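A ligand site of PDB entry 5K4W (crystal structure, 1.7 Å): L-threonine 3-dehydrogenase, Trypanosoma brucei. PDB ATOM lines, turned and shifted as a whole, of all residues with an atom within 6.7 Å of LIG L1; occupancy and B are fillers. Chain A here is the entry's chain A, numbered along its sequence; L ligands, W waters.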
ATOM      1  N   GLN A  13     -17.118   6.810 -13.384  1.00  0.00           N
ATOM      2  CA  GLN A  13     -15.967   5.996 -13.757  1.00  0.00           C
ATOM      3  C   GLN A  13     -16.423   4.708 -14.430  1.00  0.00           C
ATOM      4  O   GLN A  13     -15.929   4.371 -15.530  1.00  0.00           O
ATOM      5  CB  GLN A  13     -15.128   5.682 -12.549  1.00  0.00           C
ATOM      6  CG  GLN A  13     -13.843   5.006 -12.959  1.00  0.00           C
ATOM      7  CD  GLN A  13     -13.101   4.403 -11.830  1.00  0.00           C
ATOM      8  OE1 GLN A  13     -13.386   4.630 -10.674  1.00  0.00           O
ATOM      9  NE2 GLN A  13     -12.096   3.681 -12.170  1.00  0.00           N
ATOM     10  N   MET A  81     -19.922   6.922  -2.723  1.00  0.00           N
ATOM     11  CA  MET A  81     -19.038   5.868  -2.302  1.00  0.00           C
ATOM     12  C   MET A  81     -18.324   6.185  -0.973  1.00  0.00           C
ATOM     13  O   MET A  81     -18.770   7.093  -0.230  1.00  0.00           O
ATOM     14  CB  MET A  81     -18.047   5.534  -3.427  1.00  0.00           C
ATOM     15  CG  MET A  81     -18.748   4.964  -4.635  1.00  0.00           C
ATOM     16  SD  MET A  81     -17.705   4.657  -6.059  1.00  0.00           S
ATOM     17  CE  MET A  81     -17.327   6.341  -6.538  1.00  0.00           C
ATOM     18  N   SER A  82     -17.305   5.416  -0.614  1.00  0.00           N
ATOM     19  CA  SER A  82     -16.902   5.358   0.785  1.00  0.00           C
ATOM     20  C   SER A  82     -16.473   6.632   1.401  1.00  0.00           C
ATOM     21  O   SER A  82     -17.114   7.122   2.350  1.00  0.00           O
ATOM     22  CB  SER A  82     -15.866   4.261   1.007  1.00  0.00           C
ATOM     23  OG  SER A  82     -14.746   4.478   0.189  1.00  0.00           O
ATOM     24  N   VAL A  83     -15.427   7.244   0.824  1.00  0.00           N
ATOM     25  CA  VAL A  83     -14.921   8.474   1.466  1.00  0.00           C
ATOM     26  C   VAL A  83     -15.968   9.595   1.387  1.00  0.00           C
ATOM     27  O   VAL A  83     -16.247  10.285   2.382  1.00  0.00           O
ATOM     28  CB  VAL A  83     -13.551   8.876   0.879  1.00  0.00           C
ATOM     29  CG1 VAL A  83     -13.085  10.237   1.418  1.00  0.00           C
ATOM     30  CG2 VAL A  83     -12.539   7.794   1.229  1.00  0.00           C
ATOM     31  N   SER A 118     -22.718  -4.205  -5.932  1.00  0.00           N
ATOM     32  CA  SER A 118     -22.281  -4.056  -4.538  1.00  0.00           C
ATOM     33  C   SER A 118     -20.760  -3.839  -4.539  1.00  0.00           C
ATOM     34  O   SER A 118     -20.157  -3.483  -5.580  1.00  0.00           O
ATOM     35  CB  SER A 118     -22.718  -5.257  -3.717  1.00  0.00           C
ATOM     36  OG  SER A 118     -22.471  -5.014  -2.363  1.00  0.00           O
ATOM     37  N   THR A 119     -20.133  -4.049  -3.395  1.00  0.00           N
ATOM     38  CA  THR A 119     -18.800  -3.593  -3.217  1.00  0.00           C
ATOM     39  C   THR A 119     -18.146  -4.310  -2.075  1.00  0.00           C
ATOM     40  O   THR A 119     -18.796  -4.808  -1.160  1.00  0.00           O
ATOM     41  CB  THR A 119     -18.784  -2.076  -2.914  1.00  0.00           C
ATOM     42  OG1 THR A 119     -17.466  -1.688  -2.514  1.00  0.00           O
ATOM     43  CG2 THR A 119     -19.749  -1.671  -1.888  1.00  0.00           C
ATOM     44  N   ILE A 120     -16.822  -4.372  -2.134  1.00  0.00           N
ATOM     45  CA  ILE A 120     -16.050  -4.811  -0.953  1.00  0.00           C
ATOM     46  C   ILE A 120     -16.316  -3.991   0.294  1.00  0.00           C
ATOM     47  O   ILE A 120     -16.146  -4.526   1.389  1.00  0.00           O
ATOM     48  CB  ILE A 120     -14.535  -4.812  -1.250  1.00  0.00           C
ATOM     49  CG1 ILE A 120     -14.069  -3.482  -1.785  1.00  0.00           C
ATOM     50  CG2 ILE A 120     -14.192  -5.960  -2.192  1.00  0.00           C
ATOM     51  CD1 ILE A 120     -12.562  -3.315  -1.836  1.00  0.00           C
ATOM     52  N   ALA A 121     -16.735  -2.731   0.131  1.00  0.00           N
ATOM     53  CA  ALA A 121     -17.153  -1.880   1.250  1.00  0.00           C
ATOM     54  C   ALA A 121     -18.329  -2.432   2.069  1.00  0.00           C
ATOM     55  O   ALA A 121     -18.604  -1.953   3.174  1.00  0.00           O
ATOM     56  CB  ALA A 121     -17.433  -0.470   0.756  1.00  0.00           C
ATOM     57  N   TYR A 144     -21.782   4.130   3.302  1.00  0.00           N
ATOM     58  CA  TYR A 144     -21.837   3.564   1.943  1.00  0.00           C
ATOM     59  C   TYR A 144     -22.013   2.012   2.001  1.00  0.00           C
ATOM     60  O   TYR A 144     -22.965   1.455   1.390  1.00  0.00           O
ATOM     61  CB  TYR A 144     -20.570   3.853   1.220  1.00  0.00           C
ATOM     62  CG  TYR A 144     -20.309   3.139  -0.074  1.00  0.00           C
ATOM     63  CD1 TYR A 144     -21.189   3.156  -1.146  1.00  0.00           C
ATOM     64  CD2 TYR A 144     -19.090   2.526  -0.255  1.00  0.00           C
ATOM     65  CE1 TYR A 144     -20.854   2.567  -2.377  1.00  0.00           C
ATOM     66  CE2 TYR A 144     -18.697   1.973  -1.459  1.00  0.00           C
ATOM     67  CZ  TYR A 144     -19.566   1.967  -2.493  1.00  0.00           C
ATOM     68  OH  TYR A 144     -19.218   1.456  -3.669  1.00  0.00           O
ATOM     69  N   LEU A 171     -17.963  -5.621  -6.232  1.00  0.00           N
ATOM     70  CA  LEU A 171     -16.802  -5.207  -7.001  1.00  0.00           C
ATOM     71  C   LEU A 171     -15.678  -4.805  -6.040  1.00  0.00           C
ATOM     72  O   LEU A 171     -15.931  -4.230  -4.987  1.00  0.00           O
ATOM     73  CB  LEU A 171     -17.170  -3.980  -7.833  1.00  0.00           C
ATOM     74  CG  LEU A 171     -18.058  -4.274  -9.043  1.00  0.00           C
ATOM     75  CD1 LEU A 171     -18.465  -2.982  -9.737  1.00  0.00           C
ATOM     76  CD2 LEU A 171     -17.390  -5.270  -9.994  1.00  0.00           C
ATOM     77  N   PRO A 172     -14.440  -5.073  -6.448  1.00  0.00           N
ATOM     78  CA  PRO A 172     -13.240  -4.620  -5.813  1.00  0.00           C
ATOM     79  C   PRO A 172     -13.000  -3.186  -6.253  1.00  0.00           C
ATOM     80  O   PRO A 172     -13.765  -2.621  -7.024  1.00  0.00           O
ATOM     81  CB  PRO A 172     -12.215  -5.576  -6.332  1.00  0.00           C
ATOM     82  CG  PRO A 172     -12.629  -5.825  -7.717  1.00  0.00           C
ATOM     83  CD  PRO A 172     -14.158  -5.826  -7.671  1.00  0.00           C
ATOM     84  N   GLY A 173     -11.895  -2.603  -5.852  1.00  0.00           N
ATOM     85  CA  GLY A 173     -11.527  -1.317  -6.433  1.00  0.00           C
ATOM     86  C   GLY A 173     -11.239  -1.393  -7.905  1.00  0.00           C
ATOM     87  O   GLY A 173     -10.523  -2.278  -8.373  1.00  0.00           O
ATOM     88  N   ILE A 174     -11.858  -0.487  -8.666  1.00  0.00           N
ATOM     89  CA  ILE A 174     -11.776  -0.545 -10.130  1.00  0.00           C
ATOM     90  C   ILE A 174     -10.816   0.558 -10.592  1.00  0.00           C
ATOM     91  O   ILE A 174     -10.927   1.750 -10.227  1.00  0.00           O
ATOM     92  CB  ILE A 174     -13.173  -0.396 -10.813  1.00  0.00           C
ATOM     93  CG1 ILE A 174     -14.163  -1.436 -10.279  1.00  0.00           C
ATOM     94  CG2 ILE A 174     -13.014  -0.460 -12.317  1.00  0.00           C
ATOM     95  CD1 ILE A 174     -13.685  -2.876 -10.349  1.00  0.00           C
ATOM     96  N   PRO A 181     -12.060   9.151 -10.731  1.00  0.00           N
ATOM     97  CA  PRO A 181     -12.994   8.406  -9.822  1.00  0.00           C
ATOM     98  C   PRO A 181     -13.790   9.304  -8.930  1.00  0.00           C
ATOM     99  O   PRO A 181     -13.466  10.497  -8.821  1.00  0.00           O
ATOM    100  CB  PRO A 181     -12.052   7.588  -8.971  1.00  0.00           C
ATOM    101  CG  PRO A 181     -10.685   8.269  -9.070  1.00  0.00           C
ATOM    102  CD  PRO A 181     -10.640   8.910 -10.406  1.00  0.00           C
ATOM    103  N   GLY A 183     -14.644   9.495  -5.462  1.00  0.00           N
ATOM    104  CA  GLY A 183     -14.485   9.771  -4.005  1.00  0.00           C
ATOM    105  C   GLY A 183     -14.606   8.508  -3.154  1.00  0.00           C
ATOM    106  O   GLY A 183     -15.418   8.430  -2.185  1.00  0.00           O
ATOM    107  N   GLY A 184     -13.895   7.483  -3.573  1.00  0.00           N
ATOM    108  CA  GLY A 184     -13.785   6.218  -2.802  1.00  0.00           C
ATOM    109  C   GLY A 184     -12.375   6.138  -2.225  1.00  0.00           C
ATOM    110  O   GLY A 184     -11.482   6.960  -2.552  1.00  0.00           O
ATOM    111  N   ALA A 185     -12.147   5.152  -1.364  1.00  0.00           N
ATOM    112  CA  ALA A 185     -10.864   4.981  -0.736  1.00  0.00           C
ATOM    113  C   ALA A 185      -9.815   4.441  -1.701  1.00  0.00           C
ATOM    114  O   ALA A 185      -8.618   4.565  -1.439  1.00  0.00           O
ATOM    115  CB  ALA A 185     -11.004   4.039   0.438  1.00  0.00           C
ATOM    116  N   THR A 186     -10.239   3.766  -2.780  1.00  0.00           N
ATOM    117  CA  THR A 186      -9.256   3.190  -3.692  1.00  0.00           C
ATOM    118  C   THR A 186      -8.773   4.171  -4.750  1.00  0.00           C
ATOM    119  O   THR A 186      -7.938   3.847  -5.573  1.00  0.00           O
ATOM    120  CB  THR A 186      -9.842   1.993  -4.427  1.00  0.00           C
ATOM    121  OG1 THR A 186     -11.028   2.431  -5.116  1.00  0.00           O
ATOM    122  CG2 THR A 186     -10.215   0.889  -3.482  1.00  0.00           C
ATOM    123  N   ASP A 187      -9.272   5.394  -4.700  1.00  0.00           N
ATOM    124  CA  ASP A 187      -8.909   6.432  -5.698  1.00  0.00           C
ATOM    125  C   ASP A 187      -7.408   6.764  -5.721  1.00  0.00           C
ATOM    126  O   ASP A 187      -6.887   7.144  -6.783  1.00  0.00           O
ATOM    127  CB  ASP A 187      -9.689   7.708  -5.402  1.00  0.00           C
ATOM    128  CG  ASP A 187     -11.200   7.565  -5.599  1.00  0.00           C
ATOM    129  OD1 ASP A 187     -11.696   6.422  -5.686  1.00  0.00           O
ATOM    130  OD2 ASP A 187     -11.882   8.667  -5.633  1.00  0.00           O
ATOM    131  N   PRO A 213      -8.402  -5.807  -2.670  1.00  0.00           N
ATOM    132  CA  PRO A 213      -8.783  -6.435  -3.890  1.00  0.00           C
ATOM    133  C   PRO A 213      -8.968  -5.312  -4.943  1.00  0.00           C
ATOM    134  O   PRO A 213      -9.645  -4.245  -4.594  1.00  0.00           O
ATOM    135  CB  PRO A 213     -10.146  -7.082  -3.533  1.00  0.00           C
ATOM    136  CG  PRO A 213     -10.144  -7.199  -2.058  1.00  0.00           C
ATOM    137  CD  PRO A 213      -9.354  -6.056  -1.575  1.00  0.00           C
ATOM    138  N   ILE A 276     -10.813   3.422   6.566  1.00  0.00           N
ATOM    139  CA  ILE A 276     -11.846   2.661   5.758  1.00  0.00           C
ATOM    140  C   ILE A 276     -11.260   1.396   5.134  1.00  0.00           C
ATOM    141  O   ILE A 276     -11.780   0.296   5.310  1.00  0.00           O
ATOM    142  CB  ILE A 276     -12.383   3.600   4.682  1.00  0.00           C
ATOM    143  CG1 ILE A 276     -13.277   4.632   5.378  1.00  0.00           C
ATOM    144  CG2 ILE A 276     -13.212   2.804   3.648  1.00  0.00           C
ATOM    145  CD1 ILE A 276     -13.614   5.758   4.424  1.00  0.00           C
ATOM    146  N   TRP A 280     -11.598  -3.412   5.338  1.00  0.00           N
ATOM    147  CA  TRP A 280     -12.093  -4.185   4.215  1.00  0.00           C
ATOM    148  C   TRP A 280     -11.191  -5.413   4.042  1.00  0.00           C
ATOM    149  O   TRP A 280     -10.099  -5.430   4.575  1.00  0.00           O
ATOM    150  CB  TRP A 280     -11.955  -3.389   2.937  1.00  0.00           C
ATOM    151  CG  TRP A 280     -12.889  -2.196   2.878  1.00  0.00           C
ATOM    152  CD1 TRP A 280     -13.951  -1.953   3.657  1.00  0.00           C
ATOM    153  CD2 TRP A 280     -12.866  -1.144   1.867  1.00  0.00           C
ATOM    154  NE1 TRP A 280     -14.548  -0.773   3.236  1.00  0.00           N
ATOM    155  CE2 TRP A 280     -13.924  -0.299   2.104  1.00  0.00           C
ATOM    156  CE3 TRP A 280     -12.054  -0.898   0.767  1.00  0.00           C
ATOM    157  CZ2 TRP A 280     -14.199   0.839   1.296  1.00  0.00           C
ATOM    158  CZ3 TRP A 280     -12.297   0.207  -0.043  1.00  0.00           C
ATOM    159  CH2 TRP A 280     -13.376   1.070   0.228  1.00  0.00           C
HETATM  160  N1  LIG L   1     -13.949   2.614  -5.134  1.00  0.00           N
HETATM  161  C1  LIG L   1     -15.030   2.415  -4.137  1.00  0.00           C
HETATM  162  C2  LIG L   1     -14.557   2.946  -2.821  1.00  0.00           C
HETATM  163  O1  LIG L   1     -15.442   3.319  -2.064  1.00  0.00           O
HETATM  164  C3  LIG L   1     -15.464   0.961  -4.147  1.00  0.00           C
HETATM  165  O2  LIG L   1     -16.633   0.775  -3.368  1.00  0.00           O
HETATM  166  C4  LIG L   1     -14.290   0.049  -3.737  1.00  0.00           C
HETATM  167  O3  LIG L   1     -13.307   3.065  -2.668  1.00  0.00           O
HETATM  168  P1  LG2 L   2     -18.962   7.633  -9.983  1.00  0.00           P
HETATM  169  O1  LG2 L   2     -17.657   7.781 -10.828  1.00  0.00           O
HETATM  170  O2  LG2 L   2     -19.070   8.480  -8.730  1.00  0.00           O
HETATM  171  O3  LG2 L   2     -20.334   7.778 -10.879  1.00  0.00           O
HETATM  172  C1  LG2 L   2     -21.574   7.942 -10.177  1.00  0.00           C
HETATM  173  C2  LG2 L   2     -22.397   8.588 -11.303  1.00  0.00           C
HETATM  174  O4  LG2 L   2     -23.766   8.672 -10.816  1.00  0.00           O
HETATM  175  C3  LG2 L   2     -22.160  10.005 -11.666  1.00  0.00           C
HETATM  176  O5  LG2 L   2     -21.756  10.311 -12.950  1.00  0.00           O
HETATM  177  C4  LG2 L   2     -23.109  10.838 -10.975  1.00  0.00           C
HETATM  178  O6  LG2 L   2     -23.370  12.086 -11.672  1.00  0.00           O
HETATM  179  C5  LG2 L   2     -24.307   9.903 -11.077  1.00  0.00           C
HETATM  180  N1  LG2 L   2     -25.391  10.275 -10.121  1.00  0.00           N
HETATM  181  C6  LG2 L   2     -25.297  10.630  -8.809  1.00  0.00           C
HETATM  182  N2  LG2 L   2     -26.566  10.883  -8.378  1.00  0.00           N
HETATM  183  C7  LG2 L   2     -27.399  10.562  -9.347  1.00  0.00           C
HETATM  184  C8  LG2 L   2     -28.782  10.664  -9.447  1.00  0.00           C
HETATM  185  N3  LG2 L   2     -29.464  11.153  -8.428  1.00  0.00           N
HETATM  186  N4  LG2 L   2     -29.433  10.340 -10.590  1.00  0.00           N
HETATM  187  C9  LG2 L   2     -28.667   9.904 -11.654  1.00  0.00           C
HETATM  188  N5  LG2 L   2     -27.254   9.877 -11.582  1.00  0.00           N
HETATM  189  C10 LG2 L   2     -26.666  10.191 -10.417  1.00  0.00           C
HETATM  190  O7  LG2 L   2     -19.120   6.128  -9.436  1.00  0.00           O
HETATM  191  P2  LG2 L   2     -18.536   4.834 -10.130  1.00  0.00           P
HETATM  192  O8  LG2 L   2     -18.748   4.837 -11.620  1.00  0.00           O
HETATM  193  O9  LG2 L   2     -17.139   4.537  -9.652  1.00  0.00           O
HETATM  194  O10 LG2 L   2     -19.605   3.725  -9.489  1.00  0.00           O
HETATM  195  C11 LG2 L   2     -20.827   3.342 -10.138  1.00  0.00           C
HETATM  196  C12 LG2 L   2     -21.207   2.318  -9.143  1.00  0.00           C
HETATM  197  O11 LG2 L   2     -20.447   1.128  -9.105  1.00  0.00           O
HETATM  198  C13 LG2 L   2     -21.757   2.477  -7.791  1.00  0.00           C
HETATM  199  O12 LG2 L   2     -22.944   1.901  -7.415  1.00  0.00           O
HETATM  200  C14 LG2 L   2     -20.629   2.255  -6.986  1.00  0.00           C
HETATM  201  O13 LG2 L   2     -20.973   1.839  -5.648  1.00  0.00           O
HETATM  202  C15 LG2 L   2     -20.066   1.100  -7.821  1.00  0.00           C
HETATM  203  N6  LG2 L   2     -18.864   0.353  -7.488  1.00  0.00           N
HETATM  204  C16 LG2 L   2     -17.787   1.138  -7.852  1.00  0.00           C
HETATM  205  C17 LG2 L   2     -16.465   0.787  -7.576  1.00  0.00           C
HETATM  206  C18 LG2 L   2     -15.277   1.489  -8.004  1.00  0.00           C
HETATM  207  O14 LG2 L   2     -14.143   1.121  -7.614  1.00  0.00           O
HETATM  208  N7  LG2 L   2     -15.374   2.608  -8.794  1.00  0.00           N
HETATM  209  C19 LG2 L   2     -16.319  -0.518  -6.946  1.00  0.00           C
HETATM  210  C20 LG2 L   2     -17.475  -1.020  -6.287  1.00  0.00           C
HETATM  211  C21 LG2 L   2     -18.745  -0.602  -6.515  1.00  0.00           C
HETATM  212  O   HOH W   1     -13.809   5.055  -6.476  1.00  0.00           O
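The backbone NH of Ser 82 sits at hydrogen-bond distance from an oxygen (O1) of LIG L1 (3.2 Å).
OG of Ser 82 sits at hydrogen-bond distance from O1 of LIG L1 (2.6 Å).
O2 of LIG L1 is in hydrogen-bond range of OH of Tyr 144, 2.7 Å away.
O3 of LIG L1 sits at hydrogen-bond distance from N of Ala 185 (2.7 Å).
OG1 of Thr 119 lies within hydrogen-bond range of O2 of LIG L1, 2.7 Å away.
O3 of LIG L1 sits at hydrogen-bond distance from N of Thr 186 (3.1 Å).
The side-chain hydroxyl of Thr 186 lies within hydrogen-bond range of a nitrogen (N1) of LIG L1 (2.9 Å).
An oxygen (O13) of LG2 L2 sits at hydrogen-bond distance from the side-chain hydroxyl of Tyr 144 (2.7 Å).
N of Ile 174 sits at hydrogen-bond distance from O14 of LG2 L2, at 3.0 Å.
The backbone NH (N) of Gln 13 is in hydrogen-bond range of an oxygen (O1) of LG2 L2 (2.8 Å).
The side-chain amide oxygen (OE1) of Gln 13 sits at hydrogen-bond distance from a nitrogen (N7) of LG2 L2 (3.4 Å).
An oxygen (O14) of LG2 L2 is in hydrogen-bond range of a nitrogen (N1) of LIG L1 (2.9 Å).
The side-chain hydroxyl (OG) of Ser 82 is in hydrogen-bond range of the backbone NH (N) of Ala 185 (3.1 Å).
The side-chain hydroxyl (OG1) of Thr 119 is in hydrogen-bond range of the backbone NH (N) of Ala 121 (2.9 Å).
OD2 of Asp 187 lies within hydrogen-bond range of N of Gly 184, at 3.1 Å.
Water W1 bridges OD1 of Asp 187 (2.6 Å) and N1 of LIG L1 (2.8 Å).
Met 81 touches LIG L1 (CB to O1, 3.7 Å).
Gly 184 touches LIG L1 (CA to O3, 3.2 Å).
CH2 of Trp 280 touches O3 of LIG L1, 3.5 Å away.
Within 4 Å of LIG L1: Met 81, Ser 82, Thr 119, Tyr 144, Gly 184, Ala 185, Thr 186 and Trp 280.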
